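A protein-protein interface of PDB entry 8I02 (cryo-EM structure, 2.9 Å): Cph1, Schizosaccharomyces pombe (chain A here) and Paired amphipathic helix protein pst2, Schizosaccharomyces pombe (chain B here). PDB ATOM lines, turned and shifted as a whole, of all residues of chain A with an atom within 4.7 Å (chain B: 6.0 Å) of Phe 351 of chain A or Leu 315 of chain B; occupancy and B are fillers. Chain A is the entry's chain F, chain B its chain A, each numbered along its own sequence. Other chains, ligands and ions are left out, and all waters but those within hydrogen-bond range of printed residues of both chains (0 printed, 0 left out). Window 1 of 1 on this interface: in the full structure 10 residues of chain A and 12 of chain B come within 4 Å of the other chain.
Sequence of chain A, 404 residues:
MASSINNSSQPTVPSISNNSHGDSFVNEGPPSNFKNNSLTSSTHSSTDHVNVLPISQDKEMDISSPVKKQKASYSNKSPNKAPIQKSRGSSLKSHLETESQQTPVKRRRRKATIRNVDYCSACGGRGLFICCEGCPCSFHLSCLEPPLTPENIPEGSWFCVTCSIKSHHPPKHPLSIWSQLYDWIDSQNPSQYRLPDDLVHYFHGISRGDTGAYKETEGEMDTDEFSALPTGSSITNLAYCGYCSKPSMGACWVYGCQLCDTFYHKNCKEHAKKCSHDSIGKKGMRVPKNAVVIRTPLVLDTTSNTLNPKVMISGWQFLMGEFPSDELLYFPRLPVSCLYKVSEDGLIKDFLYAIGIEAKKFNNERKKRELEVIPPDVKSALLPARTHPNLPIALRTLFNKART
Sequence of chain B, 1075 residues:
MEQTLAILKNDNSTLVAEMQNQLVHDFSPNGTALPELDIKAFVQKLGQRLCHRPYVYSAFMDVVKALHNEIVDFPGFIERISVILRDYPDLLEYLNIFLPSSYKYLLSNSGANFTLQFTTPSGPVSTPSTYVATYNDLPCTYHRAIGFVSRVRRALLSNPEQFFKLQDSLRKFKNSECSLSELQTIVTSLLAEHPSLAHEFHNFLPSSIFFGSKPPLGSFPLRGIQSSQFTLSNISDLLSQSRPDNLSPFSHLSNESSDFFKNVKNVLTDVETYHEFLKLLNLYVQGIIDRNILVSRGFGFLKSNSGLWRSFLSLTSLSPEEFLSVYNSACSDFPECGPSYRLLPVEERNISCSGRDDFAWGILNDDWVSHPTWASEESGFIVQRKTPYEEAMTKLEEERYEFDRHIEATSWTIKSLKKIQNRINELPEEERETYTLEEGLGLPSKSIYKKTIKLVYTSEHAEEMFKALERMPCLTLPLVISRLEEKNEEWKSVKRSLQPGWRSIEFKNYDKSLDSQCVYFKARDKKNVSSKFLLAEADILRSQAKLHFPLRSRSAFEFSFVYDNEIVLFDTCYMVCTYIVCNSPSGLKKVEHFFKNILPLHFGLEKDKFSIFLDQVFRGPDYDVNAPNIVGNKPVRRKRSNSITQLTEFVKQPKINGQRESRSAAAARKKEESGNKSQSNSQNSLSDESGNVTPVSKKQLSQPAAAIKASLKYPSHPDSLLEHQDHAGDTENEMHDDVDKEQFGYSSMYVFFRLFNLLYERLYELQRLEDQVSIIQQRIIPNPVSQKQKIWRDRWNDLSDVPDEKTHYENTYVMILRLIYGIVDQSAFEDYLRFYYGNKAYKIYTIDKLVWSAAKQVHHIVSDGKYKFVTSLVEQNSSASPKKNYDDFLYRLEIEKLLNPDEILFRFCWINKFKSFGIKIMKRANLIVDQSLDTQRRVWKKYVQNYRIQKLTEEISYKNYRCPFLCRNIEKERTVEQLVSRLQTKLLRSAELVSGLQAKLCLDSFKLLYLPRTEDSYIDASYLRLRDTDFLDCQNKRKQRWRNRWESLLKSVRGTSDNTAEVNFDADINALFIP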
ATOM      1  N   LEU A 347       4.459   2.454  13.753  1.00  0.00           N
ATOM      2  CA  LEU A 347       3.991   2.873  12.439  1.00  0.00           C
ATOM      3  C   LEU A 347       2.577   3.433  12.506  1.00  0.00           C
ATOM      4  O   LEU A 347       2.276   4.458  11.887  1.00  0.00           O
ATOM      5  CB  LEU A 347       4.057   1.678  11.493  1.00  0.00           C
ATOM      6  CG  LEU A 347       4.353   1.838  10.009  1.00  0.00           C
ATOM      7  CD1 LEU A 347       4.871   0.523   9.472  1.00  0.00           C
ATOM      8  CD2 LEU A 347       3.108   2.251   9.280  1.00  0.00           C
ATOM      9  N   ILE A 348       1.698   2.778  13.264  1.00  0.00           N
ATOM     10  CA  ILE A 348       0.305   3.204  13.343  1.00  0.00           C
ATOM     11  C   ILE A 348       0.184   4.542  14.062  1.00  0.00           C
ATOM     12  O   ILE A 348      -0.607   5.407  13.667  1.00  0.00           O
ATOM     13  CB  ILE A 348      -0.526   2.112  14.031  1.00  0.00           C
ATOM     14  CG1 ILE A 348      -0.696   0.919  13.097  1.00  0.00           C
ATOM     15  CG2 ILE A 348      -1.867   2.661  14.469  1.00  0.00           C
ATOM     16  CD1 ILE A 348      -0.988  -0.369  13.803  1.00  0.00           C
ATOM     17  N   LYS A 349       0.956   4.735  15.133  1.00  0.00           N
ATOM     18  CA  LYS A 349       0.906   6.006  15.848  1.00  0.00           C
ATOM     19  C   LYS A 349       1.506   7.126  15.013  1.00  0.00           C
ATOM     20  O   LYS A 349       0.989   8.255  15.013  1.00  0.00           O
ATOM     21  CB  LYS A 349       1.613   5.878  17.190  1.00  0.00           C
ATOM     22  CG  LYS A 349       0.760   5.199  18.238  1.00  0.00           C
ATOM     23  CD  LYS A 349       1.537   4.882  19.496  1.00  0.00           C
ATOM     24  CE  LYS A 349       2.559   3.794  19.262  1.00  0.00           C
ATOM     25  NZ  LYS A 349       3.041   3.218  20.544  1.00  0.00           N
ATOM     26  N   ASP A 350       2.571   6.823  14.264  1.00  0.00           N
ATOM     27  CA  ASP A 350       3.109   7.778  13.301  1.00  0.00           C
ATOM     28  C   ASP A 350       2.059   8.193  12.285  1.00  0.00           C
ATOM     29  O   ASP A 350       1.899   9.384  11.992  1.00  0.00           O
ATOM     30  CB  ASP A 350       4.316   7.177  12.592  1.00  0.00           C
ATOM     31  CG  ASP A 350       5.558   7.217  13.436  1.00  0.00           C
ATOM     32  OD1 ASP A 350       5.465   7.651  14.598  1.00  0.00           O
ATOM     33  OD2 ASP A 350       6.629   6.823  12.937  1.00  0.00           O
ATOM     34  N   PHE A 351       1.328   7.220  11.735  1.00  0.00           N
ATOM     35  CA  PHE A 351       0.330   7.553  10.727  1.00  0.00           C
ATOM     36  C   PHE A 351      -0.788   8.399  11.314  1.00  0.00           C
ATOM     37  O   PHE A 351      -1.224   9.377  10.698  1.00  0.00           O
ATOM     38  CB  PHE A 351      -0.250   6.295  10.083  1.00  0.00           C
ATOM     39  CG  PHE A 351      -1.347   6.593   9.099  1.00  0.00           C
ATOM     40  CD1 PHE A 351      -1.067   7.252   7.917  1.00  0.00           C
ATOM     41  CD2 PHE A 351      -2.661   6.265   9.374  1.00  0.00           C
ATOM     42  CE1 PHE A 351      -2.059   7.548   7.028  1.00  0.00           C
ATOM     43  CE2 PHE A 351      -3.656   6.570   8.480  1.00  0.00           C
ATOM     44  CZ  PHE A 351      -3.350   7.210   7.311  1.00  0.00           C
ATOM     45  N   LEU A 352      -1.277   8.029  12.499  1.00  0.00           N
ATOM     46  CA  LEU A 352      -2.369   8.785  13.102  1.00  0.00           C
ATOM     47  C   LEU A 352      -1.951  10.218  13.394  1.00  0.00           C
ATOM     48  O   LEU A 352      -2.720  11.157  13.168  1.00  0.00           O
ATOM     49  CB  LEU A 352      -2.848   8.093  14.374  1.00  0.00           C
ATOM     50  CG  LEU A 352      -3.610   6.779  14.220  1.00  0.00           C
ATOM     51  CD1 LEU A 352      -3.961   6.251  15.584  1.00  0.00           C
ATOM     52  CD2 LEU A 352      -4.858   6.969  13.390  1.00  0.00           C
ATOM     53  N   TYR A 353      -0.718  10.405  13.867  1.00  0.00           N
ATOM     54  CA  TYR A 353      -0.207  11.752  14.102  1.00  0.00           C
ATOM     55  C   TYR A 353      -0.152  12.554  12.808  1.00  0.00           C
ATOM     56  O   TYR A 353      -0.671  13.678  12.735  1.00  0.00           O
ATOM     57  CB  TYR A 353       1.174  11.658  14.753  1.00  0.00           C
ATOM     58  CG  TYR A 353       1.779  12.991  15.097  1.00  0.00           C
ATOM     59  CD1 TYR A 353       1.003  14.007  15.625  1.00  0.00           C
ATOM     60  CD2 TYR A 353       3.124  13.232  14.904  1.00  0.00           C
ATOM     61  CE1 TYR A 353       1.545  15.227  15.934  1.00  0.00           C
ATOM     62  CE2 TYR A 353       3.676  14.451  15.216  1.00  0.00           C
ATOM     63  CZ  TYR A 353       2.882  15.444  15.734  1.00  0.00           C
ATOM     64  OH  TYR A 353       3.426  16.665  16.051  1.00  0.00           O
ATOM     65  N   ALA A 354       0.469  11.986  11.772  1.00  0.00           N
ATOM     66  CA  ALA A 354       0.631  12.712  10.517  1.00  0.00           C
ATOM     67  C   ALA A 354      -0.712  13.099   9.914  1.00  0.00           C
ATOM     68  O   ALA A 354      -0.903  14.235   9.457  1.00  0.00           O
ATOM     69  CB  ALA A 354       1.434  11.864   9.536  1.00  0.00           C
ATOM     70  N   ILE A 355      -1.668  12.173   9.926  1.00  0.00           N
ATOM     71  CA  ILE A 355      -2.935  12.460   9.278  1.00  0.00           C
ATOM     72  C   ILE A 355      -3.789  13.390  10.126  1.00  0.00           C
ATOM     73  O   ILE A 355      -4.567  14.174   9.580  1.00  0.00           O
ATOM     74  CB  ILE A 355      -3.671  11.159   8.918  1.00  0.00           C
ATOM     75  CG1 ILE A 355      -4.724  11.440   7.853  1.00  0.00           C
ATOM     76  CG2 ILE A 355      -4.281  10.514  10.129  1.00  0.00           C
ATOM     77  CD1 ILE A 355      -4.178  12.103   6.613  1.00  0.00           C
ATOM     78  N   GLU B 256     -12.256   5.976  17.867  1.00  0.00           N
ATOM     79  CA  GLU B 256     -12.153   5.475  16.500  1.00  0.00           C
ATOM     80  C   GLU B 256     -10.755   4.935  16.197  1.00  0.00           C
ATOM     81  O   GLU B 256     -10.601   3.984  15.434  1.00  0.00           O
ATOM     82  CB  GLU B 256     -12.511   6.576  15.503  1.00  0.00           C
ATOM     83  CG  GLU B 256     -12.547   6.108  14.057  1.00  0.00           C
ATOM     84  CD  GLU B 256     -12.469   7.252  13.074  1.00  0.00           C
ATOM     85  OE1 GLU B 256     -11.674   8.184  13.306  1.00  0.00           O
ATOM     86  OE2 GLU B 256     -13.215   7.224  12.078  1.00  0.00           O
ATOM     87  N   SER B 257      -9.739   5.560  16.798  1.00  0.00           N
ATOM     88  CA  SER B 257      -8.361   5.145  16.567  1.00  0.00           C
ATOM     89  C   SER B 257      -8.142   3.693  16.966  1.00  0.00           C
ATOM     90  O   SER B 257      -7.259   3.024  16.413  1.00  0.00           O
ATOM     91  CB  SER B 257      -7.402   6.055  17.334  1.00  0.00           C
ATOM     92  OG  SER B 257      -7.660   6.010  18.726  1.00  0.00           O
ATOM     93  N   PHE B 260     -10.516   1.632  14.124  1.00  0.00           N
ATOM     94  CA  PHE B 260     -10.086   1.411  12.752  1.00  0.00           C
ATOM     95  C   PHE B 260      -9.052   0.305  12.646  1.00  0.00           C
ATOM     96  O   PHE B 260      -9.210  -0.614  11.843  1.00  0.00           O
ATOM     97  CB  PHE B 260      -9.524   2.687  12.136  1.00  0.00           C
ATOM     98  CG  PHE B 260      -9.234   2.555  10.669  1.00  0.00           C
ATOM     99  CD1 PHE B 260      -7.968   2.252  10.221  1.00  0.00           C
ATOM    100  CD2 PHE B 260     -10.235   2.712   9.740  1.00  0.00           C
ATOM    101  CE1 PHE B 260      -7.709   2.122   8.884  1.00  0.00           C
ATOM    102  CE2 PHE B 260      -9.980   2.580   8.403  1.00  0.00           C
ATOM    103  CZ  PHE B 260      -8.715   2.283   7.976  1.00  0.00           C
ATOM    104  N   PHE B 261      -7.983   0.375  13.431  1.00  0.00           N
ATOM    105  CA  PHE B 261      -6.902  -0.579  13.243  1.00  0.00           C
ATOM    106  C   PHE B 261      -7.175  -1.926  13.892  1.00  0.00           C
ATOM    107  O   PHE B 261      -6.431  -2.877  13.632  1.00  0.00           O
ATOM    108  CB  PHE B 261      -5.592   0.016  13.751  1.00  0.00           C
ATOM    109  CG  PHE B 261      -5.021   1.052  12.836  1.00  0.00           C
ATOM    110  CD1 PHE B 261      -4.343   0.681  11.694  1.00  0.00           C
ATOM    111  CD2 PHE B 261      -5.182   2.392  13.103  1.00  0.00           C
ATOM    112  CE1 PHE B 261      -3.837   1.623  10.848  1.00  0.00           C
ATOM    113  CE2 PHE B 261      -4.668   3.338  12.259  1.00  0.00           C
ATOM    114  CZ  PHE B 261      -3.994   2.955  11.134  1.00  0.00           C
ATOM    115  N   LEU B 281       0.626   3.051   4.067  1.00  0.00           N
ATOM    116  CA  LEU B 281       0.520   4.088   5.092  1.00  0.00           C
ATOM    117  C   LEU B 281       1.888   4.649   5.469  1.00  0.00           C
ATOM    118  O   LEU B 281       2.036   5.856   5.688  1.00  0.00           O
ATOM    119  CB  LEU B 281      -0.183   3.533   6.324  1.00  0.00           C
ATOM    120  CG  LEU B 281      -1.577   2.957   6.149  1.00  0.00           C
ATOM    121  CD1 LEU B 281      -2.130   2.674   7.504  1.00  0.00           C
ATOM    122  CD2 LEU B 281      -2.458   3.914   5.422  1.00  0.00           C
ATOM    123  N   ASN B 282       2.906   3.794   5.538  1.00  0.00           N
ATOM    124  CA  ASN B 282       4.245   4.253   5.889  1.00  0.00           C
ATOM    125  C   ASN B 282       4.812   5.196   4.843  1.00  0.00           C
ATOM    126  O   ASN B 282       5.327   6.264   5.178  1.00  0.00           O
ATOM    127  CB  ASN B 282       5.183   3.073   6.068  1.00  0.00           C
ATOM    128  CG  ASN B 282       6.625   3.483   6.036  1.00  0.00           C
ATOM    129  OD1 ASN B 282       7.240   3.528   4.982  1.00  0.00           O
ATOM    130  ND2 ASN B 282       7.180   3.776   7.197  1.00  0.00           N
ATOM    131  N   TYR B 284       3.167   6.953   2.952  1.00  0.00           N
ATOM    132  CA  TYR B 284       2.494   8.235   3.125  1.00  0.00           C
ATOM    133  C   TYR B 284       3.163   9.059   4.213  1.00  0.00           C
ATOM    134  O   TYR B 284       3.320  10.276   4.074  1.00  0.00           O
ATOM    135  CB  TYR B 284       1.026   8.055   3.479  1.00  0.00           C
ATOM    136  CG  TYR B 284       0.422   9.342   3.977  1.00  0.00           C
ATOM    137  CD1 TYR B 284       0.293   9.597   5.328  1.00  0.00           C
ATOM    138  CD2 TYR B 284      -0.011  10.309   3.089  1.00  0.00           C
ATOM    139  CE1 TYR B 284      -0.244  10.770   5.774  1.00  0.00           C
ATOM    140  CE2 TYR B 284      -0.559  11.477   3.532  1.00  0.00           C
ATOM    141  CZ  TYR B 284      -0.674  11.702   4.870  1.00  0.00           C
ATOM    142  OH  TYR B 284      -1.214  12.866   5.320  1.00  0.00           O
ATOM    143  N   VAL B 285       3.506   8.412   5.329  1.00  0.00           N
ATOM    144  CA  VAL B 285       4.103   9.119   6.460  1.00  0.00           C
ATOM    145  C   VAL B 285       5.416   9.762   6.053  1.00  0.00           C
ATOM    146  O   VAL B 285       5.703  10.906   6.420  1.00  0.00           O
ATOM    147  CB  VAL B 285       4.293   8.159   7.644  1.00  0.00           C
ATOM    148  CG1 VAL B 285       5.417   8.618   8.531  1.00  0.00           C
ATOM    149  CG2 VAL B 285       3.032   8.066   8.421  1.00  0.00           C
ATOM    150  N   LEU B 294      -3.143   8.118  -1.289  1.00  0.00           N
ATOM    151  CA  LEU B 294      -3.399   7.238  -0.155  1.00  0.00           C
ATOM    152  C   LEU B 294      -4.850   6.788  -0.123  1.00  0.00           C
ATOM    153  O   LEU B 294      -5.140   5.613   0.112  1.00  0.00           O
ATOM    154  CB  LEU B 294      -3.034   7.934   1.154  1.00  0.00           C
ATOM    155  CG  LEU B 294      -3.285   7.157   2.449  1.00  0.00           C
ATOM    156  CD1 LEU B 294      -2.298   6.048   2.588  1.00  0.00           C
ATOM    157  CD2 LEU B 294      -3.221   8.074   3.632  1.00  0.00           C
ATOM    158  N   ARG B 310     -16.019   3.882   5.009  1.00  0.00           N
ATOM    159  CA  ARG B 310     -16.613   5.138   5.442  1.00  0.00           C
ATOM    160  C   ARG B 310     -15.873   5.713   6.634  1.00  0.00           C
ATOM    161  O   ARG B 310     -15.775   6.937   6.769  1.00  0.00           O
ATOM    162  CB  ARG B 310     -18.078   4.940   5.797  1.00  0.00           C
ATOM    163  CG  ARG B 310     -19.000   4.841   4.628  1.00  0.00           C
ATOM    164  CD  ARG B 310     -20.429   4.863   5.109  1.00  0.00           C
ATOM    165  NE  ARG B 310     -21.369   5.029   4.009  1.00  0.00           N
ATOM    166  CZ  ARG B 310     -22.101   4.045   3.504  1.00  0.00           C
ATOM    167  NH1 ARG B 310     -22.002   2.829   4.012  1.00  0.00           N
ATOM    168  NH2 ARG B 310     -22.932   4.280   2.499  1.00  0.00           N
ATOM    169  N   SER B 311     -15.370   4.846   7.512  1.00  0.00           N
ATOM    170  CA  SER B 311     -14.524   5.287   8.613  1.00  0.00           C
ATOM    171  C   SER B 311     -13.251   5.934   8.093  1.00  0.00           C
ATOM    172  O   SER B 311     -12.912   7.061   8.466  1.00  0.00           O
ATOM    173  CB  SER B 311     -14.192   4.093   9.501  1.00  0.00           C
ATOM    174  OG  SER B 311     -12.852   4.143   9.929  1.00  0.00           O
ATOM    175  N   PHE B 312     -12.542   5.230   7.210  1.00  0.00           N
ATOM    176  CA  PHE B 312     -11.292   5.729   6.650  1.00  0.00           C
ATOM    177  C   PHE B 312     -11.484   7.063   5.944  1.00  0.00           C
ATOM    178  O   PHE B 312     -10.597   7.916   5.975  1.00  0.00           O
ATOM    179  CB  PHE B 312     -10.728   4.691   5.692  1.00  0.00           C
ATOM    180  CG  PHE B 312      -9.344   4.981   5.218  1.00  0.00           C
ATOM    181  CD1 PHE B 312      -9.079   5.131   3.875  1.00  0.00           C
ATOM    182  CD2 PHE B 312      -8.297   5.068   6.105  1.00  0.00           C
ATOM    183  CE1 PHE B 312      -7.810   5.374   3.432  1.00  0.00           C
ATOM    184  CE2 PHE B 312      -7.023   5.309   5.656  1.00  0.00           C
ATOM    185  CZ  PHE B 312      -6.785   5.464   4.317  1.00  0.00           C
ATOM    186  N   LEU B 313     -12.629   7.262   5.298  1.00  0.00           N
ATOM    187  CA  LEU B 313     -12.865   8.535   4.628  1.00  0.00           C
ATOM    188  C   LEU B 313     -13.040   9.695   5.600  1.00  0.00           C
ATOM    189  O   LEU B 313     -12.983  10.851   5.175  1.00  0.00           O
ATOM    190  CB  LEU B 313     -14.099   8.456   3.730  1.00  0.00           C
ATOM    191  CG  LEU B 313     -14.013   7.816   2.352  1.00  0.00           C
ATOM    192  CD1 LEU B 313     -15.174   8.297   1.538  1.00  0.00           C
ATOM    193  CD2 LEU B 313     -12.725   8.167   1.676  1.00  0.00           C
ATOM    194  N   SER B 314     -13.286   9.425   6.880  1.00  0.00           N
ATOM    195  CA  SER B 314     -13.366  10.481   7.880  1.00  0.00           C
ATOM    196  C   SER B 314     -12.111  10.576   8.727  1.00  0.00           C
ATOM    197  O   SER B 314     -11.825  11.651   9.265  1.00  0.00           O
ATOM    198  CB  SER B 314     -14.563  10.260   8.808  1.00  0.00           C
ATOM    199  OG  SER B 314     -14.321   9.160   9.662  1.00  0.00           O
ATOM    200  N   LEU B 315     -11.372   9.476   8.861  1.00  0.00           N
ATOM    201  CA  LEU B 315     -10.066   9.494   9.502  1.00  0.00           C
ATOM    202  C   LEU B 315      -9.071  10.345   8.736  1.00  0.00           C
ATOM    203  O   LEU B 315      -8.076  10.780   9.319  1.00  0.00           O
ATOM    204  CB  LEU B 315      -9.556   8.066   9.633  1.00  0.00           C
ATOM    205  CG  LEU B 315      -8.208   7.708  10.224  1.00  0.00           C
ATOM    206  CD1 LEU B 315      -8.334   6.377  10.914  1.00  0.00           C
ATOM    207  CD2 LEU B 315      -7.211   7.597   9.121  1.00  0.00           C
ATOM    208  N   THR B 316      -9.318  10.588   7.448  1.00  0.00           N
ATOM    209  CA  THR B 316      -8.488  11.440   6.609  1.00  0.00           C
ATOM    210  C   THR B 316      -9.224  12.682   6.135  1.00  0.00           C
ATOM    211  O   THR B 316      -8.689  13.431   5.317  1.00  0.00           O
ATOM    212  CB  THR B 316      -7.974  10.671   5.392  1.00  0.00           C
ATOM    213  OG1 THR B 316      -8.997  10.639   4.396  1.00  0.00           O
ATOM    214  CG2 THR B 316      -7.590   9.251   5.763  1.00  0.00           C
ATOM    215  N   SER B 317     -10.449  12.902   6.604  1.00  0.00           N
ATOM    216  CA  SER B 317     -11.202  14.128   6.337  1.00  0.00           C
ATOM    217  C   SER B 317     -11.474  14.333   4.850  1.00  0.00           C
ATOM    218  O   SER B 317     -11.505  15.464   4.358  1.00  0.00           O
ATOM    219  CB  SER B 317     -10.490  15.347   6.919  1.00  0.00           C
ATOM    220  OG  SER B 317     -11.013  16.541   6.362  1.00  0.00           O
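Among the printed residues, pairs that only touch across the chains: Ile 355 of chain A with Tyr 284 of chain B (3.3 Å), Phe 351 of chain A with Tyr 284 of chain B (3.6 Å), Phe 351 of chain A with Val 285 of chain B (3.6 Å), Ile 348 of chain A with Phe 261 of chain B (3.6 Å), Phe 351 of chain A with Leu 294 of chain B (3.6 Å), Ile 355 of chain A with Leu 315 of chain B (3.7 Å), Phe 351 of chain A with Leu 315 of chain B (3.8 Å), Leu 352 of chain A with Phe 261 of chain B (3.8 Å), Leu 352 of chain A with Ser 257 of chain B (3.9 Å), Phe 351 of chain A with Leu 281 of chain B (3.9 Å), Leu 347 of chain A with Asn 282 of chain B (3.9 Å), Ile 355 of chain A with Thr 316 of chain B (3.96 Å), Asp 350 of chain A with Val 285 of chain B (3.97 Å) and Phe 351 of chain A with Phe 261 of chain B (3.98 Å).
Of the printed residues of chain B, Leu 347 of chain A touches Asn 282. Printed residues of chain B within 4 Å of Asp 350 of chain A: Val 285 (3.97 Å). Tyr 353 of chain A touches none of the printed residues of chain B. Leu 315 of chain B touches two residues of chain A. The nearest residue of chain B that does not touch Phe 351 of chain A is Phe 312 of chain B (4.5 Å).
Of the 17 printed residues of chain B, 9 touch a printed residue of chain A. Hydrophobic or aromatic side chains of chain B within 4 Å of the printed part of chain A: Phe 261, Leu 281, Tyr 284, Val 285, Leu 294 and Leu 315. Along chain B the printed residues that touch a printed residue of chain A span positions 257 to 316. Among the printed residues, 14 pairs touch across the chains.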
